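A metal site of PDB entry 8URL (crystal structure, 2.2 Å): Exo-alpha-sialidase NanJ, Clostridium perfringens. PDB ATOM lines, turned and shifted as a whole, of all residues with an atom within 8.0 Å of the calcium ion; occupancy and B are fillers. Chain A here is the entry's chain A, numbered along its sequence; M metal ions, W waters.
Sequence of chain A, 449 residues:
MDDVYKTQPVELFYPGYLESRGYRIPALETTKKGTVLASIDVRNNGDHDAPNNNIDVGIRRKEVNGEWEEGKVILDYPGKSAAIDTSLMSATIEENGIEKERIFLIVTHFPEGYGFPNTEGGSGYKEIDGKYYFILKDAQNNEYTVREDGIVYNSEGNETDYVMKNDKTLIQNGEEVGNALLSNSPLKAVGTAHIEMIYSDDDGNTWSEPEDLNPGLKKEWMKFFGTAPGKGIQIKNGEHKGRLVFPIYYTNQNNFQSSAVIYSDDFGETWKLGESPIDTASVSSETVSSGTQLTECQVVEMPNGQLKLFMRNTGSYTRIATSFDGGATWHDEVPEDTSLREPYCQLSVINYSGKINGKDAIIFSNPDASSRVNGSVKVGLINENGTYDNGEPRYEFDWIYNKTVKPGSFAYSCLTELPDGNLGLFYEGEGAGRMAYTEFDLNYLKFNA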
ATOM      1  N   VAL A  42      14.079  19.439 -10.378  1.00  0.00           N
ATOM      2  CA  VAL A  42      14.720  18.630 -11.397  1.00  0.00           C
ATOM      3  C   VAL A  42      13.632  18.287 -12.413  1.00  0.00           C
ATOM      4  O   VAL A  42      12.865  17.350 -12.211  1.00  0.00           O
ATOM      5  CB  VAL A  42      15.355  17.384 -10.804  1.00  0.00           C
ATOM      6  CG1 VAL A  42      16.076  16.565 -11.876  1.00  0.00           C
ATOM      7  CG2 VAL A  42      16.315  17.815  -9.699  1.00  0.00           C
ATOM      8  N   ASN A  44      12.799  16.783 -15.402  1.00  0.00           N
ATOM      9  CA  ASN A  44      13.549  15.850 -16.229  1.00  0.00           C
ATOM     10  C   ASN A  44      13.129  15.867 -17.682  1.00  0.00           C
ATOM     11  O   ASN A  44      13.969  15.645 -18.549  1.00  0.00           O
ATOM     12  CB  ASN A  44      13.419  14.433 -15.684  1.00  0.00           C
ATOM     13  CG  ASN A  44      14.290  14.218 -14.492  1.00  0.00           C
ATOM     14  OD1 ASN A  44      15.522  14.211 -14.614  1.00  0.00           O
ATOM     15  ND2 ASN A  44      13.676  14.068 -13.318  1.00  0.00           N
ATOM     16  N   ASN A  53       5.460  16.014 -16.687  1.00  0.00           N
ATOM     17  CA  ASN A  53       6.884  16.190 -16.438  1.00  0.00           C
ATOM     18  C   ASN A  53       7.282  15.412 -15.196  1.00  0.00           C
ATOM     19  O   ASN A  53       6.695  15.595 -14.122  1.00  0.00           O
ATOM     20  CB  ASN A  53       7.241  17.667 -16.287  1.00  0.00           C
ATOM     21  CG  ASN A  53       8.717  17.911 -16.465  1.00  0.00           C
ATOM     22  OD1 ASN A  53       9.507  16.975 -16.498  1.00  0.00           O
ATOM     23  ND2 ASN A  53       9.104  19.165 -16.548  1.00  0.00           N
ATOM     24  N   ASN A  54       8.278  14.556 -15.342  1.00  0.00           N
ATOM     25  CA  ASN A  54       8.861  13.870 -14.194  1.00  0.00           C
ATOM     26  C   ASN A  54       9.741  14.867 -13.433  1.00  0.00           C
ATOM     27  O   ASN A  54      10.935  15.004 -13.714  1.00  0.00           O
ATOM     28  CB  ASN A  54       9.642  12.644 -14.631  1.00  0.00           C
ATOM     29  CG  ASN A  54      10.411  12.005 -13.504  1.00  0.00           C
ATOM     30  OD1 ASN A  54      10.099  12.205 -12.345  1.00  0.00           O
ATOM     31  ND2 ASN A  54      11.415  11.231 -13.838  1.00  0.00           N
ATOM     32  N   ILE A  55       9.141  15.593 -12.489  1.00  0.00           N
ATOM     33  CA  ILE A  55       9.853  16.648 -11.757  1.00  0.00           C
ATOM     34  C   ILE A  55      10.157  16.139 -10.349  1.00  0.00           C
ATOM     35  O   ILE A  55       9.243  15.796  -9.591  1.00  0.00           O
ATOM     36  CB  ILE A  55       9.056  17.957 -11.698  1.00  0.00           C
ATOM     37  CG1 ILE A  55       8.638  18.425 -13.088  1.00  0.00           C
ATOM     38  CG2 ILE A  55       9.900  19.054 -11.059  1.00  0.00           C
ATOM     39  CD1 ILE A  55       7.859  19.748 -13.106  1.00  0.00           C
ATOM     40  N   ASP A  56      11.443  16.132 -10.001  1.00  0.00           N
ATOM     41  CA  ASP A  56      11.945  15.787  -8.683  1.00  0.00           C
ATOM     42  C   ASP A  56      12.559  16.993  -7.982  1.00  0.00           C
ATOM     43  O   ASP A  56      12.887  18.020  -8.605  1.00  0.00           O
ATOM     44  CB  ASP A  56      13.025  14.698  -8.778  1.00  0.00           C
ATOM     45  CG  ASP A  56      12.567  13.485  -9.544  1.00  0.00           C
ATOM     46  OD1 ASP A  56      11.457  12.987  -9.289  1.00  0.00           O
ATOM     47  OD2 ASP A  56      13.344  13.027 -10.396  1.00  0.00           O
ATOM     48  N   VAL A  57      12.748  16.850  -6.668  1.00  0.00           N
ATOM     49  CA  VAL A  57      13.459  17.846  -5.860  1.00  0.00           C
ATOM     50  C   VAL A  57      14.948  17.503  -5.872  1.00  0.00           C
ATOM     51  O   VAL A  57      15.339  16.379  -5.537  1.00  0.00           O
ATOM     52  CB  VAL A  57      12.920  17.876  -4.419  1.00  0.00           C
ATOM     53  CG1 VAL A  57      13.701  18.921  -3.613  1.00  0.00           C
ATOM     54  CG2 VAL A  57      11.416  18.187  -4.398  1.00  0.00           C
ATOM     55  N   VAL A  73      19.205  14.104  -5.969  1.00  0.00           N
ATOM     56  CA  VAL A  73      17.747  14.107  -5.903  1.00  0.00           C
ATOM     57  C   VAL A  73      17.347  13.610  -4.533  1.00  0.00           C
ATOM     58  O   VAL A  73      17.798  12.538  -4.109  1.00  0.00           O
ATOM     59  CB  VAL A  73      17.145  13.215  -7.008  1.00  0.00           C
ATOM     60  CG1 VAL A  73      15.731  12.850  -6.647  1.00  0.00           C
ATOM     61  CG2 VAL A  73      17.161  13.916  -8.331  1.00  0.00           C
ATOM     62  N   LEU A  75      13.828  13.971  -3.428  1.00  0.00           N
ATOM     63  CA  LEU A  75      12.426  13.583  -3.461  1.00  0.00           C
ATOM     64  C   LEU A  75      12.025  13.269  -4.893  1.00  0.00           C
ATOM     65  O   LEU A  75      12.261  14.079  -5.797  1.00  0.00           O
ATOM     66  CB  LEU A  75      11.525  14.674  -2.875  1.00  0.00           C
ATOM     67  CG  LEU A  75      10.058  14.305  -2.624  1.00  0.00           C
ATOM     68  CD1 LEU A  75       9.971  13.131  -1.676  1.00  0.00           C
ATOM     69  CD2 LEU A  75       9.296  15.491  -2.065  1.00  0.00           C
ATOM     70  N   ASP A  76      11.408  12.104  -5.088  1.00  0.00           N
ATOM     71  CA  ASP A  76      11.208  11.524  -6.416  1.00  0.00           C
ATOM     72  C   ASP A  76       9.955  10.665  -6.354  1.00  0.00           C
ATOM     73  O   ASP A  76       9.996   9.565  -5.783  1.00  0.00           O
ATOM     74  CB  ASP A  76      12.427  10.701  -6.814  1.00  0.00           C
ATOM     75  CG  ASP A  76      12.299  10.089  -8.196  1.00  0.00           C
ATOM     76  OD1 ASP A  76      11.206  10.126  -8.790  1.00  0.00           O
ATOM     77  OD2 ASP A  76      13.317   9.589  -8.699  1.00  0.00           O
ATOM     78  N   TYR A  77       8.856  11.138  -6.937  1.00  0.00           N
ATOM     79  CA  TYR A  77       7.595  10.414  -6.976  1.00  0.00           C
ATOM     80  C   TYR A  77       7.512   9.545  -8.226  1.00  0.00           C
ATOM     81  O   TYR A  77       8.224   9.767  -9.204  1.00  0.00           O
ATOM     82  CB  TYR A  77       6.429  11.409  -6.943  1.00  0.00           C
ATOM     83  CG  TYR A  77       6.254  12.114  -5.605  1.00  0.00           C
ATOM     84  CD1 TYR A  77       5.875  11.404  -4.465  1.00  0.00           C
ATOM     85  CD2 TYR A  77       6.475  13.473  -5.481  1.00  0.00           C
ATOM     86  CE1 TYR A  77       5.719  12.027  -3.256  1.00  0.00           C
ATOM     87  CE2 TYR A  77       6.308  14.106  -4.269  1.00  0.00           C
ATOM     88  CZ  TYR A  77       5.944  13.380  -3.164  1.00  0.00           C
ATOM     89  OH  TYR A  77       5.788  14.004  -1.954  1.00  0.00           O
ATOM     90  N   PRO A  78       6.641   8.529  -8.224  1.00  0.00           N
ATOM     91  CA  PRO A  78       6.531   7.620  -9.384  1.00  0.00           C
ATOM     92  C   PRO A  78       6.155   8.338 -10.671  1.00  0.00           C
ATOM     93  O   PRO A  78       5.438   9.347 -10.668  1.00  0.00           O
ATOM     94  CB  PRO A  78       5.419   6.657  -8.979  1.00  0.00           C
ATOM     95  CG  PRO A  78       5.371   6.710  -7.480  1.00  0.00           C
ATOM     96  CD  PRO A  78       5.812   8.095  -7.089  1.00  0.00           C
ATOM     97  N   GLY A  79       6.634   7.785 -11.789  1.00  0.00           N
ATOM     98  CA  GLY A  79       6.186   8.248 -13.099  1.00  0.00           C
ATOM     99  C   GLY A  79       6.403   9.736 -13.281  1.00  0.00           C
ATOM    100  O   GLY A  79       7.359  10.314 -12.772  1.00  0.00           O
ATOM    101  N   LYS A  80       5.480  10.369 -13.994  1.00  0.00           N
ATOM    102  CA  LYS A  80       5.495  11.827 -14.158  1.00  0.00           C
ATOM    103  C   LYS A  80       4.585  12.521 -13.147  1.00  0.00           C
ATOM    104  O   LYS A  80       3.891  13.504 -13.455  1.00  0.00           O
ATOM    105  CB  LYS A  80       5.129  12.202 -15.588  1.00  0.00           C
ATOM    106  CG  LYS A  80       6.158  11.667 -16.595  1.00  0.00           C
ATOM    107  CD  LYS A  80       5.928  12.204 -17.996  1.00  0.00           C
ATOM    108  CE  LYS A  80       7.024  11.694 -18.939  1.00  0.00           C
ATOM    109  NZ  LYS A  80       6.726  12.004 -20.368  1.00  0.00           N
ATOM    110  N   SER A  81       4.539  11.978 -11.932  1.00  0.00           N
ATOM    111  CA  SER A  81       3.936  12.657 -10.794  1.00  0.00           C
ATOM    112  C   SER A  81       4.949  13.665 -10.265  1.00  0.00           C
ATOM    113  O   SER A  81       6.087  13.294  -9.952  1.00  0.00           O
ATOM    114  CB  SER A  81       3.542  11.632  -9.734  1.00  0.00           C
ATOM    115  OG  SER A  81       3.108  12.271  -8.545  1.00  0.00           O
ATOM    116  N   ALA A  82       4.554  14.933 -10.168  1.00  0.00           N
ATOM    117  CA  ALA A  82       5.527  16.010 -10.030  1.00  0.00           C
ATOM    118  C   ALA A  82       5.672  16.465  -8.585  1.00  0.00           C
ATOM    119  O   ALA A  82       4.686  16.594  -7.856  1.00  0.00           O
ATOM    120  CB  ALA A  82       5.110  17.200 -10.892  1.00  0.00           C
ATOM    121  N   ALA A  83       6.901  16.705  -8.176  1.00  0.00           N
ATOM    122  CA  ALA A  83       7.199  17.534  -7.016  1.00  0.00           C
ATOM    123  C   ALA A  83       7.764  18.840  -7.571  1.00  0.00           C
ATOM    124  O   ALA A  83       8.824  18.842  -8.195  1.00  0.00           O
ATOM    125  CB  ALA A  83       8.177  16.855  -6.070  1.00  0.00           C
HETATM  126 CA    CA M   1       9.866  11.208 -10.219  1.00  0.00          CA
HETATM  127  O   HOH W   1       8.598  12.957  -9.243  1.00  0.00           O
HETATM  128  O   HOH W   2       9.714   9.235 -11.862  1.00  0.00           O
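O of Gly 79 lies close to OD1 of Asn 54, 3.4 Å away. O of Asn 54 sits at hydrogen-bond distance from ND2 of Asn 44 (2.9 Å). The side-chain carboxylate (OD2) of Asp 56 sits at hydrogen-bond distance from the side-chain amide nitrogen (ND2) of Asn 44 (3.1 Å). The backbone carbonyl oxygen of Asp 56 is in hydrogen-bond range of the backbone NH of Val 42, at 2.6 Å.
Gly 79 touches the calcium ion (O to CA, 3.7 Å). Of the 17 residues printed, 5 come within 4 Å of the calcium ion. The nearest printed residue that does not touch the calcium ion is Ser 81 (4.3 Å).
The calcium ion is bound by OD1 of Asp 76 (2.2 Å). The calcium ion is bound by OD1 of Asn 54 (2.4 Å). The calcium ion is bound by water W1, 2.4 Å away. The calcium ion is bound by the backbone carbonyl oxygen (O) of Tyr 77, 2.4 Å away. The calcium ion is bound by OD1 of Asp 56 (2.6 Å). Water W2 binds the calcium ion, at 2.6 Å. The calcium ion has six donor atoms within binding distance.
Water W1 lies within hydrogen-bond range of O of Ser 81 (2.6 Å), O of Ile 55 (2.9 Å) and N of Tyr 77 (2.9 Å). Water W2 lies within hydrogen-bond range of O of Gly 79 (2.7 Å) and ND2 of Asn 54 (3.3 Å).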
